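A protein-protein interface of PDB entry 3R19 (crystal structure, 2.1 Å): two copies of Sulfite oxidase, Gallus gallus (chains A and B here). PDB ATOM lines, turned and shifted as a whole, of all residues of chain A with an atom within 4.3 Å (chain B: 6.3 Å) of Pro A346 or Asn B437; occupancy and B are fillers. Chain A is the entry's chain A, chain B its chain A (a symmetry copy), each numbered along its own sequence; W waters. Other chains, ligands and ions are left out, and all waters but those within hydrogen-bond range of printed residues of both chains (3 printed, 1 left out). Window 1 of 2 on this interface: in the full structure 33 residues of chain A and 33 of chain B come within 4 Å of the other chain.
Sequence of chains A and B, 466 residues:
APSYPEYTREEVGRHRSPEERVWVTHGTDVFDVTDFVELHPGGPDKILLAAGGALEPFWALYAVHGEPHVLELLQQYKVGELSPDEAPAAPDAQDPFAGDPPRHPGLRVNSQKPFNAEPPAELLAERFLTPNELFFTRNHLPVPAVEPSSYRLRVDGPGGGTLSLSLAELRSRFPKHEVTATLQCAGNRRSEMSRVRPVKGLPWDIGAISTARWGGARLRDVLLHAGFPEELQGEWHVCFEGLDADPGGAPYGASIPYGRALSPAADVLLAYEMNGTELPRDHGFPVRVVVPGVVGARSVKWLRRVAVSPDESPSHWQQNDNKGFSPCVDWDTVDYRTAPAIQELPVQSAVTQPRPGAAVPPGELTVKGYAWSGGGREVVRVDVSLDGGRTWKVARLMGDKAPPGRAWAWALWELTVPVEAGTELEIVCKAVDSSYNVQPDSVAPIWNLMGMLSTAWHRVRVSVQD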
ATOM      1  N   LEU A 345       0.588  20.940 -14.096  1.00  0.00           N
ATOM      2  CA  LEU A 345       1.288  20.522 -12.887  1.00  0.00           C
ATOM      3  C   LEU A 345       2.073  19.226 -13.131  1.00  0.00           C
ATOM      4  O   LEU A 345       1.678  18.404 -13.952  1.00  0.00           O
ATOM      5  CB  LEU A 345       0.299  20.316 -11.729  1.00  0.00           C
ATOM      6  CG  LEU A 345      -0.274  21.564 -11.039  1.00  0.00           C
ATOM      7  CD1 LEU A 345      -1.400  21.158 -10.080  1.00  0.00           C
ATOM      8  CD2 LEU A 345       0.816  22.316 -10.272  1.00  0.00           C
ATOM      9  N   PRO A 346       3.169  19.022 -12.385  1.00  0.00           N
ATOM     10  CA  PRO A 346       3.921  17.773 -12.512  1.00  0.00           C
ATOM     11  C   PRO A 346       3.245  16.613 -11.772  1.00  0.00           C
ATOM     12  O   PRO A 346       2.274  16.825 -11.029  1.00  0.00           O
ATOM     13  CB  PRO A 346       5.264  18.110 -11.864  1.00  0.00           C
ATOM     14  CG  PRO A 346       4.881  19.110 -10.758  1.00  0.00           C
ATOM     15  CD  PRO A 346       3.706  19.903 -11.328  1.00  0.00           C
ATOM     16  N   VAL A 347       3.777  15.408 -11.968  1.00  0.00           N
ATOM     17  CA  VAL A 347       3.242  14.180 -11.399  1.00  0.00           C
ATOM     18  C   VAL A 347       3.283  14.230  -9.858  1.00  0.00           C
ATOM     19  O   VAL A 347       4.242  14.732  -9.263  1.00  0.00           O
ATOM     20  CB  VAL A 347       4.001  12.942 -11.972  1.00  0.00           C
ATOM     21  CG1 VAL A 347       5.520  13.000 -11.639  1.00  0.00           C
ATOM     22  CG2 VAL A 347       3.354  11.616 -11.506  1.00  0.00           C
ATOM     23  N   GLN A 348       2.227  13.720  -9.238  1.00  0.00           N
ATOM     24  CA  GLN A 348       1.973  13.877  -7.809  1.00  0.00           C
ATOM     25  C   GLN A 348       1.301  12.612  -7.256  1.00  0.00           C
ATOM     26  O   GLN A 348       0.567  11.940  -7.984  1.00  0.00           O
ATOM     27  CB  GLN A 348       1.044  15.088  -7.603  1.00  0.00           C
ATOM     28  CG  GLN A 348       0.599  15.347  -6.155  1.00  0.00           C
ATOM     29  CD  GLN A 348       1.753  15.772  -5.267  1.00  0.00           C
ATOM     30  OE1 GLN A 348       2.583  14.953  -4.871  1.00  0.00           O
ATOM     31  NE2 GLN A 348       1.819  17.066  -4.958  1.00  0.00           N
ATOM     32  N   TRP A 372      -1.803  11.577  -9.484  1.00  0.00           N
ATOM     33  CA  TRP A 372      -2.325  12.409 -10.564  1.00  0.00           C
ATOM     34  C   TRP A 372      -1.170  13.103 -11.278  1.00  0.00           C
ATOM     35  O   TRP A 372      -0.090  13.279 -10.714  1.00  0.00           O
ATOM     36  CB  TRP A 372      -3.312  13.433  -9.988  1.00  0.00           C
ATOM     37  CG  TRP A 372      -3.932  14.382 -10.973  1.00  0.00           C
ATOM     38  CD1 TRP A 372      -5.055  14.175 -11.742  1.00  0.00           C
ATOM     39  CD2 TRP A 372      -3.466  15.697 -11.292  1.00  0.00           C
ATOM     40  NE1 TRP A 372      -5.314  15.293 -12.516  1.00  0.00           N
ATOM     41  CE2 TRP A 372      -4.351  16.237 -12.260  1.00  0.00           C
ATOM     42  CE3 TRP A 372      -2.388  16.476 -10.851  1.00  0.00           C
ATOM     43  CZ2 TRP A 372      -4.184  17.521 -12.792  1.00  0.00           C
ATOM     44  CZ3 TRP A 372      -2.221  17.756 -11.389  1.00  0.00           C
ATOM     45  CH2 TRP A 372      -3.123  18.265 -12.338  1.00  0.00           C
ATOM     46  N   SER A 373      -1.401  13.502 -12.520  1.00  0.00           N
ATOM     47  CA  SER A 373      -0.423  14.304 -13.221  1.00  0.00           C
ATOM     48  C   SER A 373      -1.147  15.302 -14.120  1.00  0.00           C
ATOM     49  O   SER A 373      -2.293  15.056 -14.539  1.00  0.00           O
ATOM     50  CB  SER A 373       0.529  13.396 -14.003  1.00  0.00           C
ATOM     51  OG  SER A 373       1.622  14.135 -14.493  1.00  0.00           O
ATOM     52  N   ARG A 377      -1.894  13.869 -18.734  1.00  0.00           N
ATOM     53  CA  ARG A 377      -0.996  12.721 -18.673  1.00  0.00           C
ATOM     54  C   ARG A 377      -1.450  11.715 -17.617  1.00  0.00           C
ATOM     55  O   ARG A 377      -1.562  12.026 -16.427  1.00  0.00           O
ATOM     56  CB  ARG A 377       0.448  13.167 -18.423  1.00  0.00           C
ATOM     57  CG  ARG A 377       1.053  13.984 -19.612  1.00  0.00           C
ATOM     58  CD  ARG A 377       2.500  14.373 -19.322  1.00  0.00           C
ATOM     59  NE  ARG A 377       2.554  15.421 -18.300  1.00  0.00           N
ATOM     60  CZ  ARG A 377       2.389  16.715 -18.582  1.00  0.00           C
ATOM     61  NH1 ARG A 377       2.189  17.104 -19.831  1.00  0.00           N
ATOM     62  NH2 ARG A 377       2.434  17.618 -17.625  1.00  0.00           N
ATOM     63  N   ASN A 437       7.387  10.900 -16.586  1.00  0.00           N
ATOM     64  CA  ASN A 437       7.822  11.771 -15.506  1.00  0.00           C
ATOM     65  C   ASN A 437       7.672  11.080 -14.176  1.00  0.00           C
ATOM     66  O   ASN A 437       6.747  10.295 -13.986  1.00  0.00           O
ATOM     67  CB  ASN A 437       6.998  13.040 -15.457  1.00  0.00           C
ATOM     68  CG  ASN A 437       7.402  14.012 -16.516  1.00  0.00           C
ATOM     69  OD1 ASN A 437       6.587  14.366 -17.377  1.00  0.00           O
ATOM     70  ND2 ASN A 437       8.662  14.434 -16.491  1.00  0.00           N
ATOM     71  N   LEU A 453       4.585  23.587  -5.488  1.00  0.00           N
ATOM     72  CA  LEU A 453       5.089  22.419  -6.223  1.00  0.00           C
ATOM     73  C   LEU A 453       5.804  21.418  -5.277  1.00  0.00           C
ATOM     74  O   LEU A 453       6.989  21.070  -5.451  1.00  0.00           O
ATOM     75  CB  LEU A 453       5.996  22.904  -7.374  1.00  0.00           C
ATOM     76  CG  LEU A 453       5.254  23.785  -8.399  1.00  0.00           C
ATOM     77  CD1 LEU A 453       6.202  24.652  -9.181  1.00  0.00           C
ATOM     78  CD2 LEU A 453       4.377  22.940  -9.349  1.00  0.00           C
ATOM     79  N   THR A 455       6.062  17.949  -4.482  1.00  0.00           N
ATOM     80  CA  THR A 455       5.803  16.638  -5.095  1.00  0.00           C
ATOM     81  C   THR A 455       6.897  15.582  -4.809  1.00  0.00           C
ATOM     82  O   THR A 455       6.986  14.559  -5.501  1.00  0.00           O
ATOM     83  CB  THR A 455       5.654  16.754  -6.632  1.00  0.00           C
ATOM     84  OG1 THR A 455       6.913  17.112  -7.208  1.00  0.00           O
ATOM     85  CG2 THR A 455       4.585  17.784  -7.026  1.00  0.00           C
ATOM     86  N   VAL B 347      11.898  15.093 -18.296  1.00  0.00           N
ATOM     87  CA  VAL B 347      12.917  16.131 -18.235  1.00  0.00           C
ATOM     88  C   VAL B 347      14.299  15.520 -17.922  1.00  0.00           C
ATOM     89  O   VAL B 347      14.417  14.594 -17.114  1.00  0.00           O
ATOM     90  CB  VAL B 347      12.509  17.231 -17.204  1.00  0.00           C
ATOM     91  CG1 VAL B 347      12.343  16.640 -15.775  1.00  0.00           C
ATOM     92  CG2 VAL B 347      13.494  18.423 -17.230  1.00  0.00           C
ATOM     93  N   SER B 373      13.470  18.420 -22.445  1.00  0.00           N
ATOM     94  CA  SER B 373      12.315  17.689 -21.974  1.00  0.00           C
ATOM     95  C   SER B 373      11.434  17.323 -23.165  1.00  0.00           C
ATOM     96  O   SER B 373      11.462  18.008 -24.203  1.00  0.00           O
ATOM     97  CB  SER B 373      11.567  18.516 -20.926  1.00  0.00           C
ATOM     98  OG  SER B 373      10.588  17.731 -20.287  1.00  0.00           O
ATOM     99  N   ARG B 377       7.840  20.466 -24.209  1.00  0.00           N
ATOM    100  CA  ARG B 377       7.943  21.219 -22.964  1.00  0.00           C
ATOM    101  C   ARG B 377       9.321  21.861 -22.816  1.00  0.00           C
ATOM    102  O   ARG B 377      10.356  21.187 -22.804  1.00  0.00           O
ATOM    103  CB  ARG B 377       7.617  20.333 -21.758  1.00  0.00           C
ATOM    104  CG  ARG B 377       6.125  19.866 -21.725  1.00  0.00           C
ATOM    105  CD  ARG B 377       5.849  19.015 -20.489  1.00  0.00           C
ATOM    106  NE  ARG B 377       6.476  17.698 -20.622  1.00  0.00           N
ATOM    107  CZ  ARG B 377       5.911  16.692 -21.292  1.00  0.00           C
ATOM    108  NH1 ARG B 377       4.722  16.850 -21.852  1.00  0.00           N
ATOM    109  NH2 ARG B 377       6.522  15.530 -21.394  1.00  0.00           N
ATOM    110  N   ALA B 431      17.188  19.905 -14.041  1.00  0.00           N
ATOM    111  CA  ALA B 431      16.389  20.796 -14.874  1.00  0.00           C
ATOM    112  C   ALA B 431      14.918  20.729 -14.522  1.00  0.00           C
ATOM    113  O   ALA B 431      14.442  19.725 -13.975  1.00  0.00           O
ATOM    114  CB  ALA B 431      16.603  20.482 -16.368  1.00  0.00           C
ATOM    115  N   VAL B 432      14.210  21.804 -14.871  1.00  0.00           N
ATOM    116  CA  VAL B 432      12.788  21.977 -14.622  1.00  0.00           C
ATOM    117  C   VAL B 432      12.129  22.355 -15.942  1.00  0.00           C
ATOM    118  O   VAL B 432      12.579  23.288 -16.604  1.00  0.00           O
ATOM    119  CB  VAL B 432      12.564  23.122 -13.616  1.00  0.00           C
ATOM    120  CG1 VAL B 432      11.082  23.336 -13.331  1.00  0.00           C
ATOM    121  CG2 VAL B 432      13.319  22.852 -12.308  1.00  0.00           C
ATOM    122  N   ASP B 433      11.037  21.679 -16.318  1.00  0.00           N
ATOM    123  CA  ASP B 433      10.373  22.030 -17.585  1.00  0.00           C
ATOM    124  C   ASP B 433       9.122  22.908 -17.435  1.00  0.00           C
ATOM    125  O   ASP B 433       8.790  23.333 -16.315  1.00  0.00           O
ATOM    126  CB  ASP B 433      10.154  20.778 -18.469  1.00  0.00           C
ATOM    127  CG  ASP B 433       8.964  19.934 -18.036  1.00  0.00           C
ATOM    128  OD1 ASP B 433       8.161  20.385 -17.184  1.00  0.00           O
ATOM    129  OD2 ASP B 433       8.815  18.818 -18.585  1.00  0.00           O
ATOM    130  N   SER B 434       8.438  23.199 -18.547  1.00  0.00           N
ATOM    131  CA  SER B 434       7.303  24.145 -18.532  1.00  0.00           C
ATOM    132  C   SER B 434       6.050  23.603 -17.813  1.00  0.00           C
ATOM    133  O   SER B 434       5.152  24.360 -17.484  1.00  0.00           O
ATOM    134  CB  SER B 434       6.957  24.614 -19.955  1.00  0.00           C
ATOM    135  OG  SER B 434       6.754  23.475 -20.779  1.00  0.00           O
ATOM    136  N   SER B 435       6.004  22.303 -17.541  1.00  0.00           N
ATOM    137  CA  SER B 435       4.958  21.774 -16.683  1.00  0.00           C
ATOM    138  C   SER B 435       5.470  21.633 -15.239  1.00  0.00           C
ATOM    139  O   SER B 435       4.835  20.969 -14.400  1.00  0.00           O
ATOM    140  CB  SER B 435       4.421  20.431 -17.222  1.00  0.00           C
ATOM    141  OG  SER B 435       3.574  19.811 -16.266  1.00  0.00           O
ATOM    142  N   TYR B 436       6.620  22.260 -14.966  1.00  0.00           N
ATOM    143  CA  TYR B 436       7.337  22.109 -13.693  1.00  0.00           C
ATOM    144  C   TYR B 436       7.656  20.659 -13.274  1.00  0.00           C
ATOM    145  O   TYR B 436       7.730  20.343 -12.068  1.00  0.00           O
ATOM    146  CB  TYR B 436       6.620  22.861 -12.569  1.00  0.00           C
ATOM    147  CG  TYR B 436       6.787  24.357 -12.639  1.00  0.00           C
ATOM    148  CD1 TYR B 436       7.904  24.976 -12.067  1.00  0.00           C
ATOM    149  CD2 TYR B 436       5.830  25.154 -13.258  1.00  0.00           C
ATOM    150  CE1 TYR B 436       8.074  26.349 -12.126  1.00  0.00           C
ATOM    151  CE2 TYR B 436       5.985  26.540 -13.327  1.00  0.00           C
ATOM    152  CZ  TYR B 436       7.111  27.124 -12.748  1.00  0.00           C
ATOM    153  OH  TYR B 436       7.268  28.478 -12.768  1.00  0.00           O
ATOM    154  N   ASN B 437       7.846  19.776 -14.255  1.00  0.00           N
ATOM    155  CA  ASN B 437       8.462  18.491 -13.966  1.00  0.00           C
ATOM    156  C   ASN B 437       9.913  18.670 -13.601  1.00  0.00           C
ATOM    157  O   ASN B 437      10.579  19.555 -14.127  1.00  0.00           O
ATOM    158  CB  ASN B 437       8.403  17.569 -15.165  1.00  0.00           C
ATOM    159  CG  ASN B 437       7.046  16.973 -15.347  1.00  0.00           C
ATOM    160  OD1 ASN B 437       6.406  17.192 -16.383  1.00  0.00           O
ATOM    161  ND2 ASN B 437       6.576  16.240 -14.344  1.00  0.00           N
ATOM    162  N   VAL B 438      10.399  17.782 -12.745  1.00  0.00           N
ATOM    163  CA  VAL B 438      11.744  17.874 -12.189  1.00  0.00           C
ATOM    164  C   VAL B 438      12.429  16.519 -12.296  1.00  0.00           C
ATOM    165  O   VAL B 438      11.787  15.519 -12.616  1.00  0.00           O
ATOM    166  CB  VAL B 438      11.695  18.297 -10.696  1.00  0.00           C
ATOM    167  CG1 VAL B 438      11.117  19.698 -10.559  1.00  0.00           C
ATOM    168  CG2 VAL B 438      10.862  17.293  -9.883  1.00  0.00           C
ATOM    169  N   GLN B 439      13.734  16.495 -12.037  1.00  0.00           N
ATOM    170  CA  GLN B 439      14.511  15.257 -12.043  1.00  0.00           C
ATOM    171  C   GLN B 439      14.653  14.730 -10.623  1.00  0.00           C
ATOM    172  O   GLN B 439      14.733  15.523  -9.682  1.00  0.00           O
ATOM    173  CB  GLN B 439      15.896  15.510 -12.637  1.00  0.00           C
ATOM    174  CG  GLN B 439      15.888  15.875 -14.125  1.00  0.00           C
ATOM    175  CD  GLN B 439      17.275  16.172 -14.641  1.00  0.00           C
ATOM    176  OE1 GLN B 439      17.582  17.319 -14.994  1.00  0.00           O
ATOM    177  NE2 GLN B 439      18.145  15.145 -14.665  1.00  0.00           N
HETATM  178  O   HOH W   1      10.425  13.714 -14.210  1.00  0.00           O
HETATM  179  O   HOH W   2       2.103  15.106 -22.646  1.00  0.00           O
HETATM  180  O   HOH W   3       2.729  19.668 -21.747  1.00  0.00           O
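Of the printed residues of chain B, Pro A346 touches Ser B435 (3.3 Å), Tyr B436 (3.3 Å) and Asn B437 (3.4 Å). Of the printed residues of chain B, Arg A377 touches Arg B377 and Ser B435. Printed residues of chain B within 4 Å of Asn A437: Val B347 and Asn B437. Asn B437 touches just these residues of chain A: Pro A346 (3.4 Å), Val A347 (3.8 Å) and Asn A437 (3.0 Å). The nearest printed residue of chain B that does not touch Pro A346 is Val B438 (5.2 Å).
The side-chain carboxylate (OD1) of Asp B433 is in hydrogen-bond range of the backbone NH (N) of Asn B437, at 3.0 Å. The side-chain carboxylate of Asp B433 lies within hydrogen-bond range of the backbone NH of Ser B435. N of Tyr B436 is in hydrogen-bond range of OD1 of Asp B433, 3.3 Å away. The side-chain carboxylate of Asp B433 lies within salt-bridge range of the guanidinium group of Arg B377, at 3.3 Å.
Pro A346 touches Tyr B436 (CB to O, 3.3 Å). ND2 of Asn B437 touches CB of Pro A346 (3.4 Å). Asn B437 touches Val A347 (ND2 to N, 3.8 Å). N of Val B347 touches ND2 of Asn A437 (3.8 Å). Tyr B436 touches Leu A453.
NH1 of Arg A377 lies close to NH1 of Arg B377 (3.3 Å). N of Pro A346 sits close to O of Ser B435 (3.3 Å). The guanidinium group of Arg A377 lies within hydrogen-bond range of the side-chain hydroxyl of Ser B435, at 2.8 Å. The backbone carbonyl oxygen (O) of Leu A345 sits at hydrogen-bond distance from the side-chain hydroxyl (OG) of Ser B435. The side-chain amide oxygen (OD1) of Asn B437 lies close to the side-chain amide oxygen (OD1) of Asn A437.
Hydrophobic or aromatic side chains of chain B that line the printed part of chain A: Tyr B436. Of the 10 printed residues of chain A, 6 touch a printed residue of chain B. Printed residues of chain A that touch a printed residue of chain B: Leu A345, Pro A346, Val A347, Arg A377, Asn A437 and Leu A453. Hydrophobic or aromatic side chains of chain A within 4 Å of the printed part of chain B: Pro A346 and Leu A453.
Water W1 bridges the backbone carbonyl oxygen of Val B438 and the side-chain amide nitrogen of Asn A437. Water W3 bridges NH1 of Arg A377 (3.2 Å) and NH1 of Arg B377 (3.5 Å). Water W2 bridges NH1 of Arg B377 (3.2 Å) and NH1 of Arg A377 (3.5 Å).
Val A347 touches Asn B437, and with the chains exchanged Asn A437 touches Val B347. Arg A377 touches its own counterpart, Arg B377. Asn B437 touches its own counterpart, Asn A437. Positions printed for both chains: 347, 373, 377 and 437.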
